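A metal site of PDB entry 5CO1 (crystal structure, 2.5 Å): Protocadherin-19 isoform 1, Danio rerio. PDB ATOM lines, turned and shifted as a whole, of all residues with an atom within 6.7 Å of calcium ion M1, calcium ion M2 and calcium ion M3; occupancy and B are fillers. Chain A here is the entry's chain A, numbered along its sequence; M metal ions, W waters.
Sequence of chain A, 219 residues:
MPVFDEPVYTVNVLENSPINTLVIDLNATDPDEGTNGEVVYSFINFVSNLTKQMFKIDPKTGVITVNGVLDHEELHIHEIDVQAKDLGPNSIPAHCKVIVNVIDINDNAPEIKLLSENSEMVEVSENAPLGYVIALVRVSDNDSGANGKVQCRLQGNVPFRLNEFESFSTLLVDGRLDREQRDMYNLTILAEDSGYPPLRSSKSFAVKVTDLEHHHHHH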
ATOM      1  N   GLU A  15      -1.398  14.967 -31.354  1.00  0.00           N
ATOM      2  CA  GLU A  15      -1.890  13.636 -31.654  1.00  0.00           C
ATOM      3  C   GLU A  15      -3.121  13.774 -32.513  1.00  0.00           C
ATOM      4  O   GLU A  15      -3.762  14.812 -32.510  1.00  0.00           O
ATOM      5  CB  GLU A  15      -2.162  12.795 -30.419  1.00  0.00           C
ATOM      6  CG  GLU A  15      -3.371  13.162 -29.600  1.00  0.00           C
ATOM      7  CD  GLU A  15      -3.583  12.188 -28.465  1.00  0.00           C
ATOM      8  OE1 GLU A  15      -3.496  10.956 -28.724  1.00  0.00           O
ATOM      9  OE2 GLU A  15      -3.769  12.639 -27.304  1.00  0.00           O
ATOM     10  N   ASN A  16      -3.267  12.775 -33.389  1.00  0.00           N
ATOM     11  CA  ASN A  16      -4.405  12.631 -34.289  1.00  0.00           C
ATOM     12  C   ASN A  16      -4.328  13.618 -35.433  1.00  0.00           C
ATOM     13  O   ASN A  16      -5.289  13.847 -36.155  1.00  0.00           O
ATOM     14  CB  ASN A  16      -5.729  12.740 -33.538  1.00  0.00           C
ATOM     15  CG  ASN A  16      -5.882  11.674 -32.443  1.00  0.00           C
ATOM     16  OD1 ASN A  16      -5.327  10.567 -32.523  1.00  0.00           O
ATOM     17  ND2 ASN A  16      -6.634  12.016 -31.397  1.00  0.00           N
ATOM     18  N   LEU A  70      -1.157   9.124 -35.314  1.00  0.00           N
ATOM     19  CA  LEU A  70      -0.327   9.455 -34.163  1.00  0.00           C
ATOM     20  C   LEU A  70      -1.127   9.435 -32.890  1.00  0.00           C
ATOM     21  O   LEU A  70      -1.977  10.315 -32.690  1.00  0.00           O
ATOM     22  CB  LEU A  70       0.234  10.849 -34.310  1.00  0.00           C
ATOM     23  CG  LEU A  70       1.351  11.055 -35.312  1.00  0.00           C
ATOM     24  CD1 LEU A  70       1.742  12.508 -35.274  1.00  0.00           C
ATOM     25  CD2 LEU A  70       2.550  10.182 -34.993  1.00  0.00           C
ATOM     26  N   ASP A  71      -0.794   8.523 -31.979  1.00  0.00           N
ATOM     27  CA  ASP A  71      -1.553   8.340 -30.741  1.00  0.00           C
ATOM     28  C   ASP A  71      -0.617   8.494 -29.577  1.00  0.00           C
ATOM     29  O   ASP A  71       0.311   7.702 -29.429  1.00  0.00           O
ATOM     30  CB  ASP A  71      -2.209   6.972 -30.734  1.00  0.00           C
ATOM     31  CG  ASP A  71      -3.057   6.720 -29.471  1.00  0.00           C
ATOM     32  OD1 ASP A  71      -3.252   7.624 -28.641  1.00  0.00           O
ATOM     33  OD2 ASP A  71      -3.503   5.566 -29.321  1.00  0.00           O
ATOM     34  N   HIS A  72      -0.812   9.578 -28.810  1.00  0.00           N
ATOM     35  CA  HIS A  72      -0.034   9.818 -27.598  1.00  0.00           C
ATOM     36  C   HIS A  72      -0.089   8.639 -26.619  1.00  0.00           C
ATOM     37  O   HIS A  72       0.864   8.385 -25.871  1.00  0.00           O
ATOM     38  CB  HIS A  72      -0.546  11.062 -26.883  1.00  0.00           C
ATOM     39  CG  HIS A  72       0.102  11.308 -25.560  1.00  0.00           C
ATOM     40  ND1 HIS A  72       1.226  12.080 -25.424  1.00  0.00           N
ATOM     41  CD2 HIS A  72      -0.229  10.895 -24.314  1.00  0.00           C
ATOM     42  CE1 HIS A  72       1.552  12.167 -24.141  1.00  0.00           C
ATOM     43  NE2 HIS A  72       0.682  11.458 -23.450  1.00  0.00           N
ATOM     44  N   GLU A  73      -1.245   7.996 -26.542  1.00  0.00           N
ATOM     45  CA  GLU A  73      -1.436   6.933 -25.539  1.00  0.00           C
ATOM     46  C   GLU A  73      -0.661   5.649 -25.962  1.00  0.00           C
ATOM     47  O   GLU A  73      -0.212   4.880 -25.110  1.00  0.00           O
ATOM     48  CB  GLU A  73      -2.926   6.675 -25.302  1.00  0.00           C
ATOM     49  CG  GLU A  73      -3.614   7.784 -24.506  1.00  0.00           C
ATOM     50  CD  GLU A  73      -3.825   9.102 -25.285  1.00  0.00           C
ATOM     51  OE1 GLU A  73      -4.262   9.070 -26.466  1.00  0.00           O
ATOM     52  OE2 GLU A  73      -3.578  10.191 -24.695  1.00  0.00           O
ATOM     53  N   GLU A  74      -0.387   5.535 -27.263  1.00  0.00           N
ATOM     54  CA  GLU A  74       0.475   4.501 -27.824  1.00  0.00           C
ATOM     55  C   GLU A  74       1.971   4.823 -27.720  1.00  0.00           C
ATOM     56  O   GLU A  74       2.761   3.934 -27.483  1.00  0.00           O
ATOM     57  CB  GLU A  74       0.070   4.297 -29.278  1.00  0.00           C
ATOM     58  CG  GLU A  74       0.749   3.154 -30.009  1.00  0.00           C
ATOM     59  CD  GLU A  74       0.458   3.170 -31.515  1.00  0.00           C
ATOM     60  OE1 GLU A  74       0.850   2.224 -32.218  1.00  0.00           O
ATOM     61  OE2 GLU A  74      -0.162   4.155 -31.995  1.00  0.00           O
ATOM     62  N   ILE A 103       1.815  15.481 -28.909  1.00  0.00           N
ATOM     63  CA  ILE A 103       1.221  16.226 -27.833  1.00  0.00           C
ATOM     64  C   ILE A 103      -0.175  15.726 -27.524  1.00  0.00           C
ATOM     65  O   ILE A 103      -0.950  15.434 -28.409  1.00  0.00           O
ATOM     66  CB  ILE A 103       1.376  17.731 -28.095  1.00  0.00           C
ATOM     67  CG1 ILE A 103       2.830  18.044 -27.778  1.00  0.00           C
ATOM     68  CG2 ILE A 103       0.518  18.564 -27.137  1.00  0.00           C
ATOM     69  CD1 ILE A 103       3.373  19.130 -28.627  1.00  0.00           C
ATOM     70  N   ASP A 104      -0.393  15.462 -26.254  1.00  0.00           N
ATOM     71  CA  ASP A 104      -1.609  14.794 -25.816  1.00  0.00           C
ATOM     72  C   ASP A 104      -2.776  15.762 -25.878  1.00  0.00           C
ATOM     73  O   ASP A 104      -2.637  16.947 -25.523  1.00  0.00           O
ATOM     74  CB  ASP A 104      -1.437  14.264 -24.404  1.00  0.00           C
ATOM     75  CG  ASP A 104      -2.752  13.887 -23.759  1.00  0.00           C
ATOM     76  OD1 ASP A 104      -3.424  12.966 -24.289  1.00  0.00           O
ATOM     77  OD2 ASP A 104      -3.085  14.477 -22.703  1.00  0.00           O
ATOM     78  N   ILE A 105      -3.860  15.287 -26.480  1.00  0.00           N
ATOM     79  CA  ILE A 105      -5.181  15.872 -26.331  1.00  0.00           C
ATOM     80  C   ILE A 105      -6.185  14.982 -25.620  1.00  0.00           C
ATOM     81  O   ILE A 105      -5.960  13.778 -25.420  1.00  0.00           O
ATOM     82  CB  ILE A 105      -5.770  16.263 -27.698  1.00  0.00           C
ATOM     83  CG1 ILE A 105      -5.864  15.040 -28.603  1.00  0.00           C
ATOM     84  CG2 ILE A 105      -4.920  17.356 -28.347  1.00  0.00           C
ATOM     85  CD1 ILE A 105      -7.189  14.901 -29.288  1.00  0.00           C
ATOM     86  N   ASN A 106      -7.281  15.597 -25.175  1.00  0.00           N
ATOM     87  CA  ASN A 106      -8.320  14.871 -24.500  1.00  0.00           C
ATOM     88  C   ASN A 106      -9.203  14.065 -25.459  1.00  0.00           C
ATOM     89  O   ASN A 106     -10.306  14.432 -25.754  1.00  0.00           O
ATOM     90  CB  ASN A 106      -9.172  15.805 -23.705  1.00  0.00           C
ATOM     91  CG  ASN A 106      -9.822  15.109 -22.537  1.00  0.00           C
ATOM     92  OD1 ASN A 106      -9.433  14.019 -22.155  1.00  0.00           O
ATOM     93  ND2 ASN A 106     -10.797  15.762 -21.938  1.00  0.00           N
ATOM     94  N   ASP A 107      -8.714  12.935 -25.904  1.00  0.00           N
ATOM     95  CA  ASP A 107      -9.504  12.039 -26.727  1.00  0.00           C
ATOM     96  C   ASP A 107      -9.920  10.767 -25.957  1.00  0.00           C
ATOM     97  O   ASP A 107     -10.210   9.764 -26.560  1.00  0.00           O
ATOM     98  CB  ASP A 107      -8.720  11.681 -28.001  1.00  0.00           C
ATOM     99  CG  ASP A 107      -7.352  11.059 -27.727  1.00  0.00           C
ATOM    100  OD1 ASP A 107      -6.780  11.287 -26.634  1.00  0.00           O
ATOM    101  OD2 ASP A 107      -6.794  10.412 -28.638  1.00  0.00           O
ATOM    102  N   ASN A 108      -9.911  10.805 -24.628  1.00  0.00           N
ATOM    103  CA  ASN A 108     -10.275   9.634 -23.815  1.00  0.00           C
ATOM    104  C   ASN A 108     -11.134  10.039 -22.665  1.00  0.00           C
ATOM    105  O   ASN A 108     -10.713  10.812 -21.813  1.00  0.00           O
ATOM    106  CB  ASN A 108      -9.039   8.923 -23.256  1.00  0.00           C
ATOM    107  CG  ASN A 108      -8.365   8.010 -24.264  1.00  0.00           C
ATOM    108  OD1 ASN A 108      -8.875   6.935 -24.549  1.00  0.00           O
ATOM    109  ND2 ASN A 108      -7.280   8.485 -24.891  1.00  0.00           N
ATOM    110  N   ALA A 109     -12.327   9.474 -22.623  1.00  0.00           N
ATOM    111  CA  ALA A 109     -13.289   9.684 -21.548  1.00  0.00           C
ATOM    112  C   ALA A 109     -12.861   8.905 -20.319  1.00  0.00           C
ATOM    113  O   ALA A 109     -12.072   7.959 -20.412  1.00  0.00           O
ATOM    114  CB  ALA A 109     -14.662   9.214 -22.000  1.00  0.00           C
ATOM    115  N   PRO A 110     -13.399   9.276 -19.151  1.00  0.00           N
ATOM    116  CA  PRO A 110     -13.058   8.526 -17.948  1.00  0.00           C
ATOM    117  C   PRO A 110     -13.711   7.164 -17.919  1.00  0.00           C
ATOM    118  O   PRO A 110     -14.855   7.058 -18.339  1.00  0.00           O
ATOM    119  CB  PRO A 110     -13.588   9.397 -16.813  1.00  0.00           C
ATOM    120  CG  PRO A 110     -13.667  10.765 -17.365  1.00  0.00           C
ATOM    121  CD  PRO A 110     -13.923  10.615 -18.835  1.00  0.00           C
ATOM    122  N   ASP A 141      -8.388   7.484 -16.517  1.00  0.00           N
ATOM    123  CA  ASP A 141      -8.392   8.145 -17.785  1.00  0.00           C
ATOM    124  C   ASP A 141      -7.020   7.887 -18.404  1.00  0.00           C
ATOM    125  O   ASP A 141      -5.990   8.224 -17.822  1.00  0.00           O
ATOM    126  CB  ASP A 141      -8.618   9.663 -17.568  1.00  0.00           C
ATOM    127  CG  ASP A 141      -9.154  10.389 -18.810  1.00  0.00           C
ATOM    128  OD1 ASP A 141      -8.459  10.398 -19.842  1.00  0.00           O
ATOM    129  OD2 ASP A 141     -10.221  11.031 -18.727  1.00  0.00           O
ATOM    130  N   ASN A 142      -7.017   7.330 -19.601  1.00  0.00           N
ATOM    131  CA  ASN A 142      -5.787   7.112 -20.336  1.00  0.00           C
ATOM    132  C   ASN A 142      -5.025   8.361 -20.787  1.00  0.00           C
ATOM    133  O   ASN A 142      -3.944   8.224 -21.323  1.00  0.00           O
ATOM    134  CB  ASN A 142      -6.039   6.238 -21.576  1.00  0.00           C
ATOM    135  CG  ASN A 142      -6.735   4.930 -21.228  1.00  0.00           C
ATOM    136  OD1 ASN A 142      -6.339   4.234 -20.310  1.00  0.00           O
ATOM    137  ND2 ASN A 142      -7.818   4.644 -21.932  1.00  0.00           N
ATOM    138  N   ASP A 143      -5.619   9.557 -20.688  1.00  0.00           N
ATOM    139  CA  ASP A 143      -4.927  10.789 -21.134  1.00  0.00           C
ATOM    140  C   ASP A 143      -3.951  11.229 -20.040  1.00  0.00           C
ATOM    141  O   ASP A 143      -4.008  10.715 -18.925  1.00  0.00           O
ATOM    142  CB  ASP A 143      -5.925  11.936 -21.462  1.00  0.00           C
ATOM    143  CG  ASP A 143      -6.899  11.590 -22.587  1.00  0.00           C
ATOM    144  OD1 ASP A 143      -6.427  11.174 -23.684  1.00  0.00           O
ATOM    145  OD2 ASP A 143      -8.133  11.751 -22.376  1.00  0.00           O
ATOM    146  N   SER A 144      -3.099  12.211 -20.344  1.00  0.00           N
ATOM    147  CA  SER A 144      -2.170  12.771 -19.357  1.00  0.00           C
ATOM    148  C   SER A 144      -2.543  14.166 -18.872  1.00  0.00           C
ATOM    149  O   SER A 144      -3.504  14.763 -19.320  1.00  0.00           O
ATOM    150  CB  SER A 144      -0.760  12.801 -19.953  1.00  0.00           C
ATOM    151  OG  SER A 144      -0.453  11.527 -20.514  1.00  0.00           O
ATOM    152  N   ALA A 146      -4.073  17.292 -16.972  1.00  0.00           N
ATOM    153  CA  ALA A 146      -5.451  17.646 -16.671  1.00  0.00           C
ATOM    154  C   ALA A 146      -6.424  16.768 -17.441  1.00  0.00           C
ATOM    155  O   ALA A 146      -7.512  16.477 -16.948  1.00  0.00           O
ATOM    156  CB  ALA A 146      -5.697  19.105 -17.040  1.00  0.00           C
ATOM    157  N   ASN A 147      -6.046  16.407 -18.661  1.00  0.00           N
ATOM    158  CA  ASN A 147      -6.928  15.610 -19.515  1.00  0.00           C
ATOM    159  C   ASN A 147      -7.233  14.290 -18.877  1.00  0.00           C
ATOM    160  O   ASN A 147      -8.165  13.595 -19.310  1.00  0.00           O
ATOM    161  CB  ASN A 147      -6.261  15.317 -20.818  1.00  0.00           C
ATOM    162  CG  ASN A 147      -6.094  16.543 -21.673  1.00  0.00           C
ATOM    163  OD1 ASN A 147      -6.929  17.438 -21.664  1.00  0.00           O
ATOM    164  ND2 ASN A 147      -5.131  16.474 -22.594  1.00  0.00           N
ATOM    165  N   GLY A 148      -6.309  13.859 -18.026  1.00  0.00           N
ATOM    166  CA  GLY A 148      -6.424  12.599 -17.311  1.00  0.00           C
ATOM    167  C   GLY A 148      -6.846  12.636 -15.845  1.00  0.00           C
ATOM    168  O   GLY A 148      -7.098  11.578 -15.292  1.00  0.00           O
ATOM    169  N   LYS A 149      -6.838  13.819 -15.196  1.00  0.00           N
ATOM    170  CA  LYS A 149      -7.387  14.020 -13.840  1.00  0.00           C
ATOM    171  C   LYS A 149      -8.909  13.972 -13.844  1.00  0.00           C
ATOM    172  O   LYS A 149      -9.544  14.847 -14.399  1.00  0.00           O
ATOM    173  CB  LYS A 149      -7.002  15.383 -13.249  1.00  0.00           C
ATOM    174  CG  LYS A 149      -5.546  15.514 -12.808  1.00  0.00           C
ATOM    175  CD  LYS A 149      -5.389  15.480 -11.277  1.00  0.00           C
ATOM    176  CE  LYS A 149      -4.091  14.787 -10.856  1.00  0.00           C
ATOM    177  NZ  LYS A 149      -2.912  15.155 -11.709  1.00  0.00           N
ATOM    178  N   VAL A 150      -9.459  13.120 -12.994  1.00  0.00           N
ATOM    179  CA  VAL A 150     -10.861  12.778 -13.030  1.00  0.00           C
ATOM    180  C   VAL A 150     -11.510  13.056 -11.689  1.00  0.00           C
ATOM    181  O   VAL A 150     -10.843  13.158 -10.694  1.00  0.00           O
ATOM    182  CB  VAL A 150     -11.007  11.283 -13.319  1.00  0.00           C
ATOM    183  CG1 VAL A 150     -12.442  10.817 -13.136  1.00  0.00           C
ATOM    184  CG2 VAL A 150     -10.528  11.024 -14.730  1.00  0.00           C
ATOM    185  N   ASP A 193     -13.499  14.480 -16.415  1.00  0.00           N
ATOM    186  CA  ASP A 193     -12.101  14.797 -16.456  1.00  0.00           C
ATOM    187  C   ASP A 193     -11.948  16.277 -16.601  1.00  0.00           C
ATOM    188  O   ASP A 193     -12.936  16.977 -16.627  1.00  0.00           O
ATOM    189  CB  ASP A 193     -11.409  14.036 -17.585  1.00  0.00           C
ATOM    190  CG  ASP A 193     -11.712  14.608 -18.949  1.00  0.00           C
ATOM    191  OD1 ASP A 193     -11.918  15.843 -19.030  1.00  0.00           O
ATOM    192  OD2 ASP A 193     -11.656  13.816 -19.931  1.00  0.00           O
ATOM    193  N   SER A 194     -10.730  16.783 -16.573  1.00  0.00           N
ATOM    194  CA  SER A 194     -10.511  18.213 -16.420  1.00  0.00           C
ATOM    195  C   SER A 194      -9.804  18.786 -17.635  1.00  0.00           C
ATOM    196  O   SER A 194      -9.168  19.837 -17.569  1.00  0.00           O
ATOM    197  CB  SER A 194      -9.695  18.461 -15.165  1.00  0.00           C
ATOM    198  OG  SER A 194     -10.270  17.727 -14.107  1.00  0.00           O
ATOM    199  N   GLY A 195      -9.865  18.045 -18.730  1.00  0.00           N
ATOM    200  CA  GLY A 195      -9.398  18.510 -20.013  1.00  0.00           C
ATOM    201  C   GLY A 195     -10.372  19.490 -20.623  1.00  0.00           C
ATOM    202  O   GLY A 195     -11.368  19.861 -20.004  1.00  0.00           O
ATOM    203  N   LEU A 199     -14.549  15.724 -20.991  1.00  0.00           N
ATOM    204  CA  LEU A 199     -15.285  14.555 -21.381  1.00  0.00           C
ATOM    205  C   LEU A 199     -15.826  13.876 -20.136  1.00  0.00           C
ATOM    206  O   LEU A 199     -15.262  13.974 -19.041  1.00  0.00           O
ATOM    207  CB  LEU A 199     -14.372  13.570 -22.105  1.00  0.00           C
ATOM    208  CG  LEU A 199     -13.873  13.917 -23.506  1.00  0.00           C
ATOM    209  CD1 LEU A 199     -12.808  12.911 -23.925  1.00  0.00           C
ATOM    210  CD2 LEU A 199     -14.999  13.935 -24.513  1.00  0.00           C
HETATM  211 CA    CA M   1      -5.094   9.128 -28.412  1.00  0.00          CA
HETATM  212 CA    CA M   2      -4.919  11.818 -25.516  1.00  0.00          CA
HETATM  213 CA    CA M   3      -9.605  12.354 -20.618  1.00  0.00          CA
HETATM  214  O   HOH W   1      -6.468   7.323 -27.631  1.00  0.00           O
HETATM  215  O   HOH W   2      -5.131   8.476 -30.583  1.00  0.00           O
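Calcium ion M1 is bound by the side-chain carboxylate (OE1) of Glu 73 (2.1 Å), the side-chain carboxylate (OD2) of Asp 107 (2.1 Å), water W2 (2.3 Å), the side-chain carboxylate (OD1) of Asp 71 (2.4 Å), water W1 (2.4 Å) and the side-chain carboxylate (OE1) of Glu 15 (2.4 Å). Calcium ion M1 has six donor atoms within binding distance.
The side-chain carboxylate (OD2) of Asp 104 lies within hydrogen-bond range of the backbone NH (N) of Ser 144 (3.3 Å). The backbone NH (N) of His 72 sits close to the side-chain carboxylate (OE1) of Glu 15, at 3.0 Å. OD2 of Asp 104 lies within hydrogen-bond range of ND2 of Asn 147 (2.9 Å). The side-chain carboxylate (OD1) of Asp 107 sits close to the side-chain amide nitrogen (ND2) of Asn 108, at 3.3 Å. N of Gly 195 is in hydrogen-bond range of OD1 of Asp 193, at 3.0 Å. The side-chain amide nitrogen (ND2) of Asn 108 sits close to the side-chain carboxylate (OE1) of Glu 73 (3.5 Å). The backbone carbonyl oxygen of Ile 103 sits at hydrogen-bond distance from the backbone NH of Glu 15. The side-chain amide nitrogen (ND2) of Asn 16 sits close to the side-chain carboxylate (OD2) of Asp 107 (3.2 Å).
Calcium ion M3 is bound by O of Asn 108 (2.2 Å), OD1 of Asn 106 (2.3 Å), O of Asn 147 (2.3 Å), OD2 of Asp 143 (2.4 Å), OD2 of Asp 141 (2.4 Å), OD1 of Asp 141 (2.4 Å) and OD2 of Asp 193 (2.6 Å). Calcium ion M3 has seven donor atoms within binding distance.
The nearest printed residue that does not touch calcium ion M1 is Asn 108 (4.2 Å).
Calcium ion M2 is bound by the backbone carbonyl oxygen of Ile 105, the side-chain carboxylate of Asp 107, the side-chain carboxylate of Asp 104, the side-chain carboxylate of Glu 73, the side-chain carboxylate of Glu 15 and the side-chain carboxylate of Asp 143. Calcium ion M2 has six donor atoms within binding distance. Slightly farther from calcium ion M2 lies OE1 of Glu 73 (3.0 Å).
Within 4 Å of calcium ion M3: Asn 106, Asn 108, Asp 141, Asp 143, Asn 147 and Asp 193.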
